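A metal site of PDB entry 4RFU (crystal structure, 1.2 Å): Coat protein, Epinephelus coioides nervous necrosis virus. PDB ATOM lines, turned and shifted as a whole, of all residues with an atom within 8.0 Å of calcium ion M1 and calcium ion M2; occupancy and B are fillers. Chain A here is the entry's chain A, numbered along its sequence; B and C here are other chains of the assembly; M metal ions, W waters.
O of Asp 60 of chain A sits at hydrogen-bond distance from OG of Ser 55 of chain A.
The backbone NH (N) of Asp 62 of chain B sits at hydrogen-bond distance from the backbone carbonyl oxygen (O) of Tyr 54 of chain B, at 2.8 Å.
The side-chain hydroxyl of Ser 55 of chain C lies within hydrogen-bond range of the backbone carbonyl oxygen of Asp 60 of chain C (2.7 Å).
The backbone carbonyl oxygen (O) of Asp 62 of chain A lies within hydrogen-bond range of the backbone NH (N) of Tyr 54 of chain A (2.8 Å).
Four residues have an atom within 4 Å of calcium ion M1: Asp 60 of chain A, Val 61 of chain A, Asp 62 of chain A and Asp 60 of chain B.
O of Val 61 of chain A binds calcium ion M1.
Calcium ion M1 is bound by OD1 of Asp 62 of chain A.
Calcium ion M1 is bound by water W1, at 2.4 Å.
The side-chain carboxylate (OD2) of Asp 60 of chain B binds calcium ion M1 (2.5 Å).
The side-chain carboxylate (OD1) of Asp 60 of chain A binds calcium ion M1, 2.5 Å away.
Calcium ion M1 is bound by the side-chain carboxylate (OD2) of Asp 60 of chain A.
Calcium ion M1 is bound by water W3 (2.5 Å).
OD1 of Asp 60 of chain B is bound to calcium ion M1, at 2.6 Å.
Calcium ion M1 has eight donor atoms within binding distance.
Calcium ion M2 is bound by OD1 of Asp 60 of chain B (2.3 Å), O of Val 61 of chain C (2.3 Å), OD1 of Asp 60 of chain C (2.4 Å), OD1 of Asp 62 of chain B (2.4 Å), water W2 (2.4 Å), water W1 (2.5 Å) and water W3 (2.5 Å).
Water W1 lies within hydrogen-bond range of OD2 of Asp 60 of chain C (2.7 Å) and OD1 of Asp 62 of chain C (2.7 Å).
Water W2 lies within hydrogen-bond range of the side-chain carboxylate of Asp 62 of chain B (2.7 Å) and the backbone NH of Val 61 of chain C (3.0 Å).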
ATOM      1  N   TYR A  54      27.842   7.461  -8.249  1.00  0.00           N
ATOM      2  CA  TYR A  54      26.645   6.956  -8.903  1.00  0.00           C
ATOM      3  C   TYR A  54      25.490   7.903  -8.627  1.00  0.00           C
ATOM      4  O   TYR A  54      25.630   8.852  -7.850  1.00  0.00           O
ATOM      5  CB  TYR A  54      26.310   5.540  -8.410  1.00  0.00           C
ATOM      6  CG  TYR A  54      25.981   5.387  -6.935  1.00  0.00           C
ATOM      7  CD1 TYR A  54      26.986   5.214  -5.983  1.00  0.00           C
ATOM      8  CD2 TYR A  54      24.654   5.361  -6.501  1.00  0.00           C
ATOM      9  CE1 TYR A  54      26.684   5.044  -4.651  1.00  0.00           C
ATOM     10  CE2 TYR A  54      24.344   5.183  -5.177  1.00  0.00           C
ATOM     11  CZ  TYR A  54      25.361   5.020  -4.250  1.00  0.00           C
ATOM     12  OH  TYR A  54      25.032   4.857  -2.922  1.00  0.00           O
ATOM     13  N   SER A  55      24.356   7.652  -9.252  1.00  0.00           N
ATOM     14  CA  SER A  55      23.159   8.441  -8.989  1.00  0.00           C
ATOM     15  C   SER A  55      21.935   7.556  -8.911  1.00  0.00           C
ATOM     16  O   SER A  55      21.692   6.736  -9.795  1.00  0.00           O
ATOM     17  CB  SER A  55      22.925   9.473 -10.084  1.00  0.00           C
ATOM     18  OG  SER A  55      21.786  10.263  -9.756  1.00  0.00           O
ATOM     19  N   LEU A  56      21.144   7.748  -7.863  1.00  0.00           N
ATOM     20  CA  LEU A  56      19.867   7.052  -7.764  1.00  0.00           C
ATOM     21  C   LEU A  56      18.724   7.879  -8.345  1.00  0.00           C
ATOM     22  O   LEU A  56      17.571   7.445  -8.348  1.00  0.00           O
ATOM     23  CB  LEU A  56      19.573   6.656  -6.321  1.00  0.00           C
ATOM     24  CG  LEU A  56      20.604   5.705  -5.715  1.00  0.00           C
ATOM     25  CD1 LEU A  56      20.204   5.276  -4.314  1.00  0.00           C
ATOM     26  CD2 LEU A  56      20.819   4.495  -6.606  1.00  0.00           C
ATOM     27  N   GLY A  57      19.035   9.072  -8.824  1.00  0.00           N
ATOM     28  CA  GLY A  57      18.027   9.946  -9.410  1.00  0.00           C
ATOM     29  C   GLY A  57      18.310  11.410  -9.159  1.00  0.00           C
ATOM     30  O   GLY A  57      19.204  11.773  -8.380  1.00  0.00           O
ATOM     31  N   GLY A  59      19.717  13.748 -10.620  1.00  0.00           N
ATOM     32  CA  GLY A  59      21.029  14.306 -10.868  1.00  0.00           C
ATOM     33  C   GLY A  59      21.910  14.396  -9.636  1.00  0.00           C
ATOM     34  O   GLY A  59      22.909  15.106  -9.638  1.00  0.00           O
ATOM     35  N   ASP A  60      21.561  13.665  -8.587  1.00  0.00           N
ATOM     36  CA  ASP A  60      22.332  13.657  -7.361  1.00  0.00           C
ATOM     37  C   ASP A  60      23.467  12.634  -7.424  1.00  0.00           C
ATOM     38  O   ASP A  60      23.291  11.533  -7.936  1.00  0.00           O
ATOM     39  CB  ASP A  60      21.434  13.340  -6.167  1.00  0.00           C
ATOM     40  CG  ASP A  60      22.225  13.058  -4.907  1.00  0.00           C
ATOM     41  OD1 ASP A  60      22.573  14.024  -4.197  1.00  0.00           O
ATOM     42  OD2 ASP A  60      22.525  11.884  -4.626  1.00  0.00           O
ATOM     43  N   VAL A  61      24.627  13.014  -6.894  1.00  0.00           N
ATOM     44  CA  VAL A  61      25.767  12.124  -6.794  1.00  0.00           C
ATOM     45  C   VAL A  61      25.839  11.487  -5.408  1.00  0.00           C
ATOM     46  O   VAL A  61      25.733  12.188  -4.397  1.00  0.00           O
ATOM     47  CB  VAL A  61      27.075  12.934  -7.002  1.00  0.00           C
ATOM     48  CG1 VAL A  61      28.309  12.061  -6.735  1.00  0.00           C
ATOM     49  CG2 VAL A  61      27.122  13.540  -8.405  1.00  0.00           C
ATOM     50  N   ASP A  62      26.041  10.173  -5.375  1.00  0.00           N
ATOM     51  CA  ASP A  62      26.429   9.422  -4.173  1.00  0.00           C
ATOM     52  C   ASP A  62      27.694   8.629  -4.518  1.00  0.00           C
ATOM     53  O   ASP A  62      28.056   8.543  -5.682  1.00  0.00           O
ATOM     54  CB  ASP A  62      25.321   8.461  -3.728  1.00  0.00           C
ATOM     55  CG  ASP A  62      24.109   9.166  -3.131  1.00  0.00           C
ATOM     56  OD1 ASP A  62      24.261  10.294  -2.608  1.00  0.00           O
ATOM     57  OD2 ASP A  62      23.016   8.583  -3.192  1.00  0.00           O
ATOM     58  N   ARG A  63      28.360   8.058  -3.523  1.00  0.00           N
ATOM     59  CA  ARG A  63      29.647   7.406  -3.773  1.00  0.00           C
ATOM     60  C   ARG A  63      29.676   5.966  -3.263  1.00  0.00           C
ATOM     61  O   ARG A  63      29.283   5.683  -2.125  1.00  0.00           O
ATOM     62  CB  ARG A  63      30.807   8.222  -3.190  1.00  0.00           C
ATOM     63  CG  ARG A  63      32.189   7.620  -3.405  1.00  0.00           C
ATOM     64  CD  ARG A  63      33.301   8.645  -3.305  1.00  0.00           C
ATOM     65  NE  ARG A  63      33.529   9.224  -4.628  1.00  0.00           N
ATOM     66  CZ  ARG A  63      34.702   9.641  -5.092  1.00  0.00           C
ATOM     67  NH1 ARG A  63      35.813   9.592  -4.370  1.00  0.00           N
ATOM     68  NH2 ARG A  63      34.756  10.153  -6.307  1.00  0.00           N
ATOM     69  N   TYR B  54      26.447   7.902   5.898  1.00  0.00           N
ATOM     70  CA  TYR B  54      25.661   8.525   6.946  1.00  0.00           C
ATOM     71  C   TYR B  54      24.719   9.544   6.337  1.00  0.00           C
ATOM     72  O   TYR B  54      24.810   9.849   5.140  1.00  0.00           O
ATOM     73  CB  TYR B  54      26.571   9.182   7.986  1.00  0.00           C
ATOM     74  CG  TYR B  54      27.362  10.373   7.463  1.00  0.00           C
ATOM     75  CD1 TYR B  54      28.598  10.207   6.856  1.00  0.00           C
ATOM     76  CD2 TYR B  54      26.885  11.665   7.616  1.00  0.00           C
ATOM     77  CE1 TYR B  54      29.329  11.294   6.385  1.00  0.00           C
ATOM     78  CE2 TYR B  54      27.594  12.754   7.155  1.00  0.00           C
ATOM     79  CZ  TYR B  54      28.818  12.566   6.545  1.00  0.00           C
ATOM     80  OH  TYR B  54      29.535  13.668   6.100  1.00  0.00           O
ATOM     81  N   LEU B  56      22.669  13.464   7.076  1.00  0.00           N
ATOM     82  CA  LEU B  56      22.347  14.659   7.853  1.00  0.00           C
ATOM     83  C   LEU B  56      20.860  14.726   8.149  1.00  0.00           C
ATOM     84  O   LEU B  56      20.421  15.555   8.950  1.00  0.00           O
ATOM     85  CB  LEU B  56      22.769  15.901   7.076  1.00  0.00           C
ATOM     86  CG  LEU B  56      24.243  16.016   6.696  1.00  0.00           C
ATOM     87  CD1 LEU B  56      24.474  17.213   5.772  1.00  0.00           C
ATOM     88  CD2 LEU B  56      25.128  16.102   7.941  1.00  0.00           C
ATOM     89  N   THR B  58      18.223  15.014   5.737  1.00  0.00           N
ATOM     90  CA  THR B  58      17.374  15.782   4.831  1.00  0.00           C
ATOM     91  C   THR B  58      17.099  15.050   3.512  1.00  0.00           C
ATOM     92  O   THR B  58      16.470  15.608   2.609  1.00  0.00           O
ATOM     93  CB  THR B  58      17.987  17.153   4.502  1.00  0.00           C
ATOM     94  OG1 THR B  58      19.302  16.957   3.974  1.00  0.00           O
ATOM     95  CG2 THR B  58      18.063  18.030   5.748  1.00  0.00           C
ATOM     96  N   GLY B  59      17.576  13.822   3.420  1.00  0.00           N
ATOM     97  CA  GLY B  59      17.278  12.983   2.273  1.00  0.00           C
ATOM     98  C   GLY B  59      18.470  12.359   1.568  1.00  0.00           C
ATOM     99  O   GLY B  59      18.258  11.541   0.673  1.00  0.00           O
ATOM    100  N   ASP B  60      19.695  12.700   1.964  1.00  0.00           N
ATOM    101  CA  ASP B  60      20.882  12.329   1.180  1.00  0.00           C
ATOM    102  C   ASP B  60      21.913  11.523   1.955  1.00  0.00           C
ATOM    103  O   ASP B  60      22.092  11.699   3.170  1.00  0.00           O
ATOM    104  CB  ASP B  60      21.560  13.591   0.638  1.00  0.00           C
ATOM    105  CG  ASP B  60      22.465  13.294  -0.538  1.00  0.00           C
ATOM    106  OD1 ASP B  60      23.582  13.855  -0.597  1.00  0.00           O
ATOM    107  OD2 ASP B  60      22.071  12.515  -1.420  1.00  0.00           O
ATOM    108  N   VAL B  61      22.616  10.647   1.242  1.00  0.00           N
ATOM    109  CA  VAL B  61      23.648   9.804   1.805  1.00  0.00           C
ATOM    110  C   VAL B  61      25.025  10.409   1.541  1.00  0.00           C
ATOM    111  O   VAL B  61      25.403  10.589   0.389  1.00  0.00           O
ATOM    112  CB  VAL B  61      23.595   8.406   1.145  1.00  0.00           C
ATOM    113  CG1 VAL B  61      24.679   7.527   1.691  1.00  0.00           C
ATOM    114  CG2 VAL B  61      22.225   7.772   1.357  1.00  0.00           C
ATOM    115  N   ASP B  62      25.753  10.736   2.610  1.00  0.00           N
ATOM    116  CA  ASP B  62      27.138  11.170   2.500  1.00  0.00           C
ATOM    117  C   ASP B  62      28.049  10.067   3.013  1.00  0.00           C
ATOM    118  O   ASP B  62      27.581   9.078   3.559  1.00  0.00           O
ATOM    119  CB  ASP B  62      27.360  12.470   3.268  1.00  0.00           C
ATOM    120  CG  ASP B  62      26.666  13.655   2.619  1.00  0.00           C
ATOM    121  OD1 ASP B  62      26.644  13.726   1.363  1.00  0.00           O
ATOM    122  OD2 ASP B  62      26.125  14.517   3.351  1.00  0.00           O
ATOM    123  N   ARG B  63      29.355  10.235   2.867  1.00  0.00           N
ATOM    124  CA  ARG B  63      30.289   9.166   3.184  1.00  0.00           C
ATOM    125  C   ARG B  63      31.391   9.649   4.114  1.00  0.00           C
ATOM    126  O   ARG B  63      31.983  10.699   3.891  1.00  0.00           O
ATOM    127  CB  ARG B  63      30.883   8.573   1.894  1.00  0.00           C
ATOM    128  CG  ARG B  63      31.934   7.501   2.086  1.00  0.00           C
ATOM    129  CD  ARG B  63      31.994   6.550   0.905  1.00  0.00           C
ATOM    130  NE  ARG B  63      30.916   5.565   0.973  1.00  0.00           N
ATOM    131  CZ  ARG B  63      30.895   4.420   0.298  1.00  0.00           C
ATOM    132  NH1 ARG B  63      31.899   4.098  -0.510  1.00  0.00           N
ATOM    133  NH2 ARG B  63      29.866   3.587   0.446  1.00  0.00           N
ATOM    134  N   TYR C  54      33.693  18.105  -0.757  1.00  0.00           N
ATOM    135  CA  TYR C  54      33.586  19.356  -1.485  1.00  0.00           C
ATOM    136  C   TYR C  54      32.106  19.665  -1.705  1.00  0.00           C
ATOM    137  O   TYR C  54      31.238  18.832  -1.445  1.00  0.00           O
ATOM    138  CB  TYR C  54      34.336  19.280  -2.827  1.00  0.00           C
ATOM    139  CG  TYR C  54      33.767  18.293  -3.824  1.00  0.00           C
ATOM    140  CD1 TYR C  54      34.189  16.963  -3.834  1.00  0.00           C
ATOM    141  CD2 TYR C  54      32.845  18.689  -4.788  1.00  0.00           C
ATOM    142  CE1 TYR C  54      33.691  16.064  -4.757  1.00  0.00           C
ATOM    143  CE2 TYR C  54      32.334  17.789  -5.722  1.00  0.00           C
ATOM    144  CZ  TYR C  54      32.750  16.483  -5.698  1.00  0.00           C
ATOM    145  OH  TYR C  54      32.246  15.592  -6.624  1.00  0.00           O
ATOM    146  N   SER C  55      31.819  20.869  -2.180  1.00  0.00           N
ATOM    147  CA  SER C  55      30.439  21.207  -2.517  1.00  0.00           C
ATOM    148  C   SER C  55      30.396  22.070  -3.767  1.00  0.00           C
ATOM    149  O   SER C  55      31.100  23.073  -3.850  1.00  0.00           O
ATOM    150  CB  SER C  55      29.749  21.942  -1.372  1.00  0.00           C
ATOM    151  OG  SER C  55      28.403  22.230  -1.731  1.00  0.00           O
ATOM    152  N   GLY C  59      24.882  23.690  -0.549  1.00  0.00           N
ATOM    153  CA  GLY C  59      25.357  23.111   0.694  1.00  0.00           C
ATOM    154  C   GLY C  59      25.424  21.594   0.654  1.00  0.00           C
ATOM    155  O   GLY C  59      25.571  20.948   1.690  1.00  0.00           O
ATOM    156  N   ASP C  60      25.296  21.019  -0.541  1.00  0.00           N
ATOM    157  CA  ASP C  60      25.366  19.581  -0.698  1.00  0.00           C
ATOM    158  C   ASP C  60      26.820  19.120  -0.741  1.00  0.00           C
ATOM    159  O   ASP C  60      27.607  19.638  -1.523  1.00  0.00           O
ATOM    160  CB  ASP C  60      24.625  19.162  -1.969  1.00  0.00           C
ATOM    161  CG  ASP C  60      24.574  17.663  -2.147  1.00  0.00           C
ATOM    162  OD1 ASP C  60      24.677  16.940  -1.136  1.00  0.00           O
ATOM    163  OD2 ASP C  60      24.419  17.215  -3.297  1.00  0.00           O
ATOM    164  N   VAL C  61      27.149  18.155   0.092  1.00  0.00           N
ATOM    165  CA  VAL C  61      28.494  17.596   0.161  1.00  0.00           C
ATOM    166  C   VAL C  61      28.644  16.417  -0.798  1.00  0.00           C
ATOM    167  O   VAL C  61      27.777  15.551  -0.859  1.00  0.00           O
ATOM    168  CB  VAL C  61      28.785  17.108   1.601  1.00  0.00           C
ATOM    169  CG1 VAL C  61      30.137  16.393   1.678  1.00  0.00           C
ATOM    170  CG2 VAL C  61      28.723  18.260   2.572  1.00  0.00           C
ATOM    171  N   ASP C  62      29.738  16.411  -1.557  1.00  0.00           N
ATOM    172  CA  ASP C  62      30.166  15.240  -2.319  1.00  0.00           C
ATOM    173  C   ASP C  62      31.601  14.949  -1.924  1.00  0.00           C
ATOM    174  O   ASP C  62      32.205  15.736  -1.191  1.00  0.00           O
ATOM    175  CB  ASP C  62      30.017  15.491  -3.823  1.00  0.00           C
ATOM    176  CG  ASP C  62      28.563  15.460  -4.272  1.00  0.00           C
ATOM    177  OD1 ASP C  62      27.839  14.524  -3.872  1.00  0.00           O
ATOM    178  OD2 ASP C  62      28.139  16.385  -4.995  1.00  0.00           O
ATOM    179  N   ARG C  63      32.153  13.831  -2.382  1.00  0.00           N
ATOM    180  CA  ARG C  63      33.481  13.423  -1.921  1.00  0.00           C
ATOM    181  C   ARG C  63      34.407  13.094  -3.083  1.00  0.00           C
ATOM    182  O   ARG C  63      34.026  12.376  -4.022  1.00  0.00           O
ATOM    183  CB  ARG C  63      33.362  12.232  -0.943  1.00  0.00           C
ATOM    184  CG  ARG C  63      34.695  11.612  -0.516  1.00  0.00           C
ATOM    185  CD  ARG C  63      34.595  10.815   0.779  1.00  0.00           C
ATOM    186  NE  ARG C  63      34.619  11.712   1.941  1.00  0.00           N
ATOM    187  CZ  ARG C  63      34.949  11.349   3.169  1.00  0.00           C
ATOM    188  NH1 ARG C  63      35.243  10.084   3.454  1.00  0.00           N
ATOM    189  NH2 ARG C  63      34.962  12.260   4.141  1.00  0.00           N
HETATM  190 CA    CA M   1      24.068  12.613  -2.837  1.00  0.00          CA
HETATM  191 CA    CA M   2      25.599  14.884  -0.425  1.00  0.00          CA
HETATM  192  O   HOH W   1      25.312  14.719  -2.907  1.00  0.00           O
HETATM  193  O   HOH W   2      25.272  16.263   1.538  1.00  0.00           O
HETATM  194  O   HOH W   3      26.029  12.534  -1.309  1.00  0.00           O
